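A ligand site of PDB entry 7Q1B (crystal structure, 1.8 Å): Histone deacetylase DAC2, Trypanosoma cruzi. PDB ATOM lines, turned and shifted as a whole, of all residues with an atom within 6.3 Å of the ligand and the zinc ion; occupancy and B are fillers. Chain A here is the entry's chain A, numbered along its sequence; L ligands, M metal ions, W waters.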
ATOM      1  N   GLU A 134     -10.148  22.528  22.707  1.00  0.00           N
ATOM      2  CA  GLU A 134      -8.780  22.667  22.202  1.00  0.00           C
ATOM      3  C   GLU A 134      -8.135  21.323  21.878  1.00  0.00           C
ATOM      4  O   GLU A 134      -7.089  21.294  21.217  1.00  0.00           O
ATOM      5  CB  GLU A 134      -7.914  23.448  23.202  1.00  0.00           C
ATOM      6  CG  GLU A 134      -7.478  22.670  24.443  1.00  0.00           C
ATOM      7  CD  GLU A 134      -8.519  22.684  25.566  1.00  0.00           C
ATOM      8  OE1 GLU A 134      -9.603  23.268  25.358  1.00  0.00           O
ATOM      9  OE2 GLU A 134      -8.237  22.114  26.654  1.00  0.00           O
ATOM     10  N   HIS A 175       3.086  18.865  28.228  1.00  0.00           N
ATOM     11  CA  HIS A 175       3.042  18.709  29.673  1.00  0.00           C
ATOM     12  C   HIS A 175       1.638  18.670  30.280  1.00  0.00           C
ATOM     13  O   HIS A 175       1.535  18.377  31.475  1.00  0.00           O
ATOM     14  CB  HIS A 175       3.853  19.832  30.349  1.00  0.00           C
ATOM     15  CG  HIS A 175       3.319  21.209  30.094  1.00  0.00           C
ATOM     16  ND1 HIS A 175       3.680  22.293  30.869  1.00  0.00           N
ATOM     17  CD2 HIS A 175       2.488  21.687  29.142  1.00  0.00           C
ATOM     18  CE1 HIS A 175       3.071  23.374  30.408  1.00  0.00           C
ATOM     19  NE2 HIS A 175       2.349  23.038  29.362  1.00  0.00           N
ATOM     20  N   HIS A 176       0.574  18.961  29.528  1.00  0.00           N
ATOM     21  CA  HIS A 176      -0.780  18.961  30.105  1.00  0.00           C
ATOM     22  C   HIS A 176      -1.469  17.600  30.077  1.00  0.00           C
ATOM     23  O   HIS A 176      -2.467  17.426  30.775  1.00  0.00           O
ATOM     24  CB  HIS A 176      -1.703  19.945  29.375  1.00  0.00           C
ATOM     25  CG  HIS A 176      -1.383  21.399  29.615  1.00  0.00           C
ATOM     26  ND1 HIS A 176      -1.306  21.953  30.872  1.00  0.00           N
ATOM     27  CD2 HIS A 176      -1.162  22.412  28.742  1.00  0.00           C
ATOM     28  CE1 HIS A 176      -1.031  23.245  30.772  1.00  0.00           C
ATOM     29  NE2 HIS A 176      -0.935  23.543  29.490  1.00  0.00           N
ATOM     30  N   GLY A 183      -5.579  17.501  27.307  1.00  0.00           N
ATOM     31  CA  GLY A 183      -5.802  18.840  27.802  1.00  0.00           C
ATOM     32  C   GLY A 183      -4.769  19.800  27.234  1.00  0.00           C
ATOM     33  O   GLY A 183      -3.639  19.390  26.973  1.00  0.00           O
ATOM     34  N   GLY A 184      -5.163  21.052  27.026  1.00  0.00           N
ATOM     35  CA  GLY A 184      -4.201  22.099  26.648  1.00  0.00           C
ATOM     36  C   GLY A 184      -3.395  21.791  25.395  1.00  0.00           C
ATOM     37  O   GLY A 184      -2.203  22.103  25.335  1.00  0.00           O
ATOM     38  N   PHE A 185      -4.039  21.178  24.384  1.00  0.00           N
ATOM     39  CA  PHE A 185      -3.439  20.735  23.121  1.00  0.00           C
ATOM     40  C   PHE A 185      -2.552  19.508  23.280  1.00  0.00           C
ATOM     41  O   PHE A 185      -1.808  19.172  22.343  1.00  0.00           O
ATOM     42  CB  PHE A 185      -2.606  21.815  22.408  1.00  0.00           C
ATOM     43  CG  PHE A 185      -3.246  23.196  22.333  1.00  0.00           C
ATOM     44  CD1 PHE A 185      -4.448  23.383  21.686  1.00  0.00           C
ATOM     45  CD2 PHE A 185      -2.590  24.299  22.853  1.00  0.00           C
ATOM     46  CE1 PHE A 185      -5.015  24.649  21.599  1.00  0.00           C
ATOM     47  CE2 PHE A 185      -3.150  25.577  22.767  1.00  0.00           C
ATOM     48  CZ  PHE A 185      -4.362  25.743  22.142  1.00  0.00           C
ATOM     49  N   CYS A 186      -2.573  18.844  24.431  1.00  0.00           N
ATOM     50  CA  CYS A 186      -1.689  17.712  24.722  1.00  0.00           C
ATOM     51  C   CYS A 186      -2.488  16.422  24.780  1.00  0.00           C
ATOM     52  O   CYS A 186      -3.509  16.342  25.488  1.00  0.00           O
ATOM     53  CB  CYS A 186      -0.953  17.907  26.042  1.00  0.00           C
ATOM     54  SG  CYS A 186       0.056  19.439  26.042  1.00  0.00           S
ATOM     55  N   ASP A 215       7.284  26.884  30.878  1.00  0.00           N
ATOM     56  CA  ASP A 215       6.108  27.296  30.122  1.00  0.00           C
ATOM     57  C   ASP A 215       5.212  28.149  31.013  1.00  0.00           C
ATOM     58  O   ASP A 215       5.189  27.986  32.237  1.00  0.00           O
ATOM     59  CB  ASP A 215       5.408  26.029  29.613  1.00  0.00           C
ATOM     60  CG  ASP A 215       4.140  26.299  28.838  1.00  0.00           C
ATOM     61  OD1 ASP A 215       3.165  26.750  29.444  1.00  0.00           O
ATOM     62  OD2 ASP A 215       4.095  26.019  27.605  1.00  0.00           O
ATOM     63  N   ALA A 216       4.446  29.072  30.404  1.00  0.00           N
ATOM     64  CA  ALA A 216       3.621  30.039  31.133  1.00  0.00           C
ATOM     65  C   ALA A 216       2.430  29.402  31.844  1.00  0.00           C
ATOM     66  O   ALA A 216       1.747  30.113  32.606  1.00  0.00           O
ATOM     67  CB  ALA A 216       3.061  31.106  30.189  1.00  0.00           C
ATOM     68  N   HIS A 217       2.137  28.139  31.583  1.00  0.00           N
ATOM     69  CA  HIS A 217       0.978  27.486  32.179  1.00  0.00           C
ATOM     70  C   HIS A 217       1.414  26.370  33.104  1.00  0.00           C
ATOM     71  O   HIS A 217       2.490  25.799  32.964  1.00  0.00           O
ATOM     72  CB  HIS A 217       0.045  26.950  31.077  1.00  0.00           C
ATOM     73  CG  HIS A 217      -0.389  28.020  30.113  1.00  0.00           C
ATOM     74  ND1 HIS A 217       0.324  28.319  28.969  1.00  0.00           N
ATOM     75  CD2 HIS A 217      -1.410  28.903  30.166  1.00  0.00           C
ATOM     76  CE1 HIS A 217      -0.269  29.310  28.327  1.00  0.00           C
ATOM     77  NE2 HIS A 217      -1.316  29.685  29.044  1.00  0.00           N
ATOM     78  N   HIS A 218       0.559  26.063  34.079  1.00  0.00           N
ATOM     79  CA  HIS A 218       0.888  25.050  35.072  1.00  0.00           C
ATOM     80  C   HIS A 218       1.147  23.699  34.401  1.00  0.00           C
ATOM     81  O   HIS A 218       0.329  23.221  33.619  1.00  0.00           O
ATOM     82  CB  HIS A 218      -0.262  24.918  36.071  1.00  0.00           C
ATOM     83  CG  HIS A 218      -0.032  23.883  37.113  1.00  0.00           C
ATOM     84  ND1 HIS A 218      -1.036  23.085  37.618  1.00  0.00           N
ATOM     85  CD2 HIS A 218       1.097  23.517  37.762  1.00  0.00           C
ATOM     86  CE1 HIS A 218      -0.541  22.273  38.521  1.00  0.00           C
ATOM     87  NE2 HIS A 218       0.755  22.516  38.639  1.00  0.00           N
ATOM     88  N   GLY A 241      -4.377  32.616  38.211  1.00  0.00           N
ATOM     89  CA  GLY A 241      -5.429  33.545  38.559  1.00  0.00           C
ATOM     90  C   GLY A 241      -6.680  33.269  37.753  1.00  0.00           C
ATOM     91  O   GLY A 241      -6.736  32.348  36.945  1.00  0.00           O
ATOM     92  N   VAL A 242      -7.689  34.110  37.999  1.00  0.00           N
ATOM     93  CA  VAL A 242      -8.980  33.955  37.360  1.00  0.00           C
ATOM     94  C   VAL A 242      -8.824  34.036  35.846  1.00  0.00           C
ATOM     95  O   VAL A 242      -8.214  34.972  35.316  1.00  0.00           O
ATOM     96  CB  VAL A 242      -9.959  35.023  37.872  1.00  0.00           C
ATOM     97  CG1 VAL A 242     -11.202  35.075  36.997  1.00  0.00           C
ATOM     98  CG2 VAL A 242     -10.321  34.746  39.323  1.00  0.00           C
ATOM     99  N   GLY A 243      -9.361  33.036  35.153  1.00  0.00           N
ATOM    100  CA  GLY A 243      -9.297  33.017  33.708  1.00  0.00           C
ATOM    101  C   GLY A 243      -7.997  32.533  33.117  1.00  0.00           C
ATOM    102  O   GLY A 243      -7.835  32.575  31.893  1.00  0.00           O
ATOM    103  N   ILE A 244      -7.058  32.054  33.943  1.00  0.00           N
ATOM    104  CA  ILE A 244      -5.753  31.605  33.472  1.00  0.00           C
ATOM    105  C   ILE A 244      -5.732  30.080  33.464  1.00  0.00           C
ATOM    106  O   ILE A 244      -5.741  29.444  34.517  1.00  0.00           O
ATOM    107  CB  ILE A 244      -4.620  32.191  34.317  1.00  0.00           C
ATOM    108  CG1 ILE A 244      -4.605  33.710  34.157  1.00  0.00           C
ATOM    109  CG2 ILE A 244      -3.289  31.575  33.893  1.00  0.00           C
ATOM    110  CD1 ILE A 244      -3.564  34.417  34.981  1.00  0.00           C
ATOM    111  N   PHE A 245      -5.678  29.511  32.259  1.00  0.00           N
ATOM    112  CA  PHE A 245      -5.624  28.067  32.071  1.00  0.00           C
ATOM    113  C   PHE A 245      -4.337  27.507  32.690  1.00  0.00           C
ATOM    114  O   PHE A 245      -3.277  28.137  32.578  1.00  0.00           O
ATOM    115  CB  PHE A 245      -5.690  27.759  30.573  1.00  0.00           C
ATOM    116  CG  PHE A 245      -5.696  26.290  30.234  1.00  0.00           C
ATOM    117  CD1 PHE A 245      -6.879  25.562  30.235  1.00  0.00           C
ATOM    118  CD2 PHE A 245      -4.516  25.648  29.884  1.00  0.00           C
ATOM    119  CE1 PHE A 245      -6.886  24.206  29.913  1.00  0.00           C
ATOM    120  CE2 PHE A 245      -4.510  24.310  29.557  1.00  0.00           C
ATOM    121  CZ  PHE A 245      -5.690  23.578  29.575  1.00  0.00           C
ATOM    122  N   PRO A 246      -4.382  26.325  33.339  1.00  0.00           N
ATOM    123  CA  PRO A 246      -5.577  25.480  33.509  1.00  0.00           C
ATOM    124  C   PRO A 246      -6.274  25.634  34.869  1.00  0.00           C
ATOM    125  O   PRO A 246      -7.111  24.781  35.210  1.00  0.00           O
ATOM    126  CB  PRO A 246      -5.004  24.067  33.387  1.00  0.00           C
ATOM    127  CG  PRO A 246      -3.682  24.184  34.073  1.00  0.00           C
ATOM    128  CD  PRO A 246      -3.166  25.603  33.760  1.00  0.00           C
ATOM    129  N   GLY A 247      -5.944  26.672  35.623  1.00  0.00           N
ATOM    130  CA  GLY A 247      -6.635  26.957  36.870  1.00  0.00           C
ATOM    131  C   GLY A 247      -6.046  26.303  38.109  1.00  0.00           C
ATOM    132  O   GLY A 247      -6.523  26.591  39.224  1.00  0.00           O
ATOM    133  N   GLY A 304       8.934  26.311  27.611  1.00  0.00           N
ATOM    134  CA  GLY A 304       7.962  26.928  26.740  1.00  0.00           C
ATOM    135  C   GLY A 304       8.167  28.431  26.639  1.00  0.00           C
ATOM    136  O   GLY A 304       8.229  29.132  27.659  1.00  0.00           O
ATOM    137  N   ASP A 306       6.010  30.591  25.722  1.00  0.00           N
ATOM    138  CA  ASP A 306       4.820  31.407  25.863  1.00  0.00           C
ATOM    139  C   ASP A 306       4.826  32.246  27.134  1.00  0.00           C
ATOM    140  O   ASP A 306       3.902  33.043  27.328  1.00  0.00           O
ATOM    141  CB  ASP A 306       3.538  30.536  25.805  1.00  0.00           C
ATOM    142  CG  ASP A 306       3.531  29.398  26.784  1.00  0.00           C
ATOM    143  OD1 ASP A 306       4.514  29.197  27.531  1.00  0.00           O
ATOM    144  OD2 ASP A 306       2.499  28.697  26.793  1.00  0.00           O
ATOM    145  N   LEU A 313      -1.248  33.643  24.160  1.00  0.00           N
ATOM    146  CA  LEU A 313      -1.899  32.673  25.037  1.00  0.00           C
ATOM    147  C   LEU A 313      -1.268  32.578  26.414  1.00  0.00           C
ATOM    148  O   LEU A 313      -1.961  32.254  27.369  1.00  0.00           O
ATOM    149  CB  LEU A 313      -1.919  31.272  24.410  1.00  0.00           C
ATOM    150  CG  LEU A 313      -2.613  31.155  23.051  1.00  0.00           C
ATOM    151  CD1 LEU A 313      -2.735  29.708  22.581  1.00  0.00           C
ATOM    152  CD2 LEU A 313      -3.970  31.829  23.115  1.00  0.00           C
ATOM    153  N   GLY A 314       0.034  32.803  26.522  1.00  0.00           N
ATOM    154  CA  GLY A 314       0.638  33.001  27.829  1.00  0.00           C
ATOM    155  C   GLY A 314       0.277  34.355  28.398  1.00  0.00           C
ATOM    156  O   GLY A 314      -0.127  35.270  27.679  1.00  0.00           O
ATOM    157  N   ALA A 346       7.760  23.322  24.707  1.00  0.00           N
ATOM    158  CA  ALA A 346       6.392  23.279  25.231  1.00  0.00           C
ATOM    159  C   ALA A 346       5.530  24.251  24.434  1.00  0.00           C
ATOM    160  O   ALA A 346       5.527  24.217  23.193  1.00  0.00           O
ATOM    161  CB  ALA A 346       6.329  23.604  26.730  1.00  0.00           C
ATOM    162  N   GLY A 347       4.801  25.118  25.120  1.00  0.00           N
ATOM    163  CA  GLY A 347       4.009  26.143  24.459  1.00  0.00           C
ATOM    164  C   GLY A 347       4.886  27.214  23.832  1.00  0.00           C
ATOM    165  O   GLY A 347       6.113  27.205  23.925  1.00  0.00           O
ATOM    166  N   GLY A 348       4.226  28.171  23.176  1.00  0.00           N
ATOM    167  CA  GLY A 348       4.914  29.265  22.496  1.00  0.00           C
ATOM    168  C   GLY A 348       4.170  29.619  21.219  1.00  0.00           C
ATOM    169  O   GLY A 348       4.171  28.844  20.263  1.00  0.00           O
ATOM    170  N   TYR A 349       3.523  30.785  21.198  1.00  0.00           N
ATOM    171  CA  TYR A 349       2.571  31.107  20.135  1.00  0.00           C
ATOM    172  C   TYR A 349       2.984  32.338  19.332  1.00  0.00           C
ATOM    173  O   TYR A 349       2.145  32.950  18.658  1.00  0.00           O
ATOM    174  CB  TYR A 349       1.178  31.233  20.749  1.00  0.00           C
ATOM    175  CG  TYR A 349       0.890  29.914  21.466  1.00  0.00           C
ATOM    176  CD1 TYR A 349       0.498  28.792  20.760  1.00  0.00           C
ATOM    177  CD2 TYR A 349       1.118  29.790  22.829  1.00  0.00           C
ATOM    178  CE1 TYR A 349       0.274  27.565  21.407  1.00  0.00           C
ATOM    179  CE2 TYR A 349       0.917  28.583  23.481  1.00  0.00           C
ATOM    180  CZ  TYR A 349       0.496  27.477  22.777  1.00  0.00           C
ATOM    181  OH  TYR A 349       0.289  26.296  23.447  1.00  0.00           O
HETATM  182  N1  LIG L   1      -0.176  25.244  27.610  1.00  0.00           N
HETATM  183  O1  LIG L   1       0.458  26.815  26.126  1.00  0.00           O
HETATM  184  C1  LIG L   1      -4.483  26.819  25.944  1.00  0.00           C
HETATM  185  C2  LIG L   1      -1.860  26.349  26.335  1.00  0.00           C
HETATM  186  C3  LIG L   1      -2.377  27.623  26.122  1.00  0.00           C
HETATM  187  C4  LIG L   1      -6.345  28.372  25.407  1.00  0.00           C
HETATM  188  N2  LIG L   1      -5.794  27.040  25.686  1.00  0.00           N
HETATM  189  C5  LIG L   1      -6.818  26.006  25.862  1.00  0.00           C
HETATM  190  C6  LIG L   1      -9.875  26.450  32.135  1.00  0.00           C
HETATM  191  C7  LIG L   1      -0.417  26.145  26.658  1.00  0.00           C
HETATM  192  O2  LIG L   1       1.083  25.089  28.176  1.00  0.00           O
HETATM  193  N3  LIG L   1      -4.119  25.536  26.145  1.00  0.00           N
HETATM  194  C8  LIG L   1      -2.813  25.334  26.330  1.00  0.00           C
HETATM  195  N4  LIG L   1      -3.676  27.878  25.941  1.00  0.00           N
HETATM  196  C9  LIG L   1      -7.184  28.871  26.577  1.00  0.00           C
HETATM  197  C10 LIG L   1      -8.166  26.601  26.268  1.00  0.00           C
HETATM  198  C11 LIG L   1      -8.035  27.775  27.225  1.00  0.00           C
HETATM  199  C12 LIG L   1      -9.406  28.302  27.615  1.00  0.00           C
HETATM  200  N5  LIG L   1     -10.387  27.229  27.782  1.00  0.00           N
HETATM  201  C13 LIG L   1     -11.357  27.461  28.852  1.00  0.00           C
HETATM  202  C14 LIG L   1     -10.824  26.823  30.098  1.00  0.00           C
HETATM  203  N6  LIG L   1     -10.286  25.247  31.608  1.00  0.00           N
HETATM  204  C15 LIG L   1     -10.860  25.490  30.387  1.00  0.00           C
HETATM  205  C16 LIG L   1     -10.192  27.456  31.216  1.00  0.00           C
HETATM  206  C17 LIG L   1      -9.858  28.774  31.517  1.00  0.00           C
HETATM  207  C18 LIG L   1      -9.237  29.069  32.727  1.00  0.00           C
HETATM  208  C19 LIG L   1      -8.944  28.053  33.630  1.00  0.00           C
HETATM  209  C20 LIG L   1      -9.261  26.733  33.344  1.00  0.00           C
HETATM  210  C21 LIG L   1     -10.111  23.943  32.219  1.00  0.00           C
HETATM  211 ZN    ZN M   1       1.787  27.010  27.827  1.00  0.00          ZN
HETATM  212  O   HOH W   1      -4.294  30.485  27.346  1.00  0.00           O
HETATM  213  O   HOH W   2     -11.218  25.671  25.641  1.00  0.00           O
HETATM  214  O   HOH W   3      -6.216  32.084  26.101  1.00  0.00           O
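Water W2 lies within hydrogen-bond range of N5 of the ligand (2.8 Å) and OE1 of Glu 134 (2.9 Å). Water W1 bridges O of Leu 313 (2.9 Å) and N4 of the ligand (3.0 Å).
NE2 of His 176 sits at hydrogen-bond distance from N1 of the ligand, at 2.6 Å. A ring nitrogen (NE2) of His 175 lies close to an oxygen (O2) of the ligand (2.7 Å). OH of Tyr 349 lies close to O1 of the ligand.
The zinc ion is bound by O2 of the ligand (2.1 Å), OD2 of Asp 306 (2.1 Å), OD1 of Asp 215 (2.1 Å), O1 of the ligand (2.2 Å), ND1 of His 217 (2.3 Å) and OD2 of Asp 215 (2.5 Å). The zinc ion has six donor atoms within binding distance.
Within 4 Å of the zinc ion: Asp 215, His 217 and Asp 306.
Glu 134 touches the ligand (CG to C5, 3.7 Å). O of Gly 184 touches C8 of the ligand, 3.4 Å away. Phe 185 touches the ligand. C of Gly 243 touches C18 of the ligand (3.7 Å). O of Ile 244 touches C19 of the ligand, at 3.6 Å. N of Phe 245 touches C18 of the ligand, 3.6 Å away. O of Pro 246 touches C20 of the ligand (3.5 Å). Gly 247 touches the ligand (N to C19, 3.9 Å). Leu 313 touches the ligand (CD1 to N4, 3.9 Å). Gly 347 touches the ligand (CA to O1, 3.98 Å). Hydrophobic or aromatic side chains within 4 Å of the ligand: His 175, His 176, Phe 185, His 217, Phe 245, Leu 313 and Tyr 349.
A ring nitrogen (NE2) of His 217 sits at hydrogen-bond distance from the backbone carbonyl oxygen (O) of Leu 313, 3.1 Å away. The backbone NH (N) of Gly 184 lies within hydrogen-bond range of the side-chain carboxylate (OE2) of Glu 134, 3.3 Å away. N of His 176 sits at hydrogen-bond distance from SG of Cys 186, at 3.6 Å. A ring nitrogen (NE2) of His 176 is in hydrogen-bond range of a ring nitrogen (NE2) of His 175, at 3.3 Å. O of His 218 lies close to ND1 of His 176. N of Ala 216 is in hydrogen-bond range of OD1 of Asp 306 (2.9 Å). O of Gly 184 sits at hydrogen-bond distance from SG of Cys 186, 3.6 Å away. The side-chain sulfur (SG) of Cys 186 lies within hydrogen-bond range of the backbone NH (N) of His 175.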
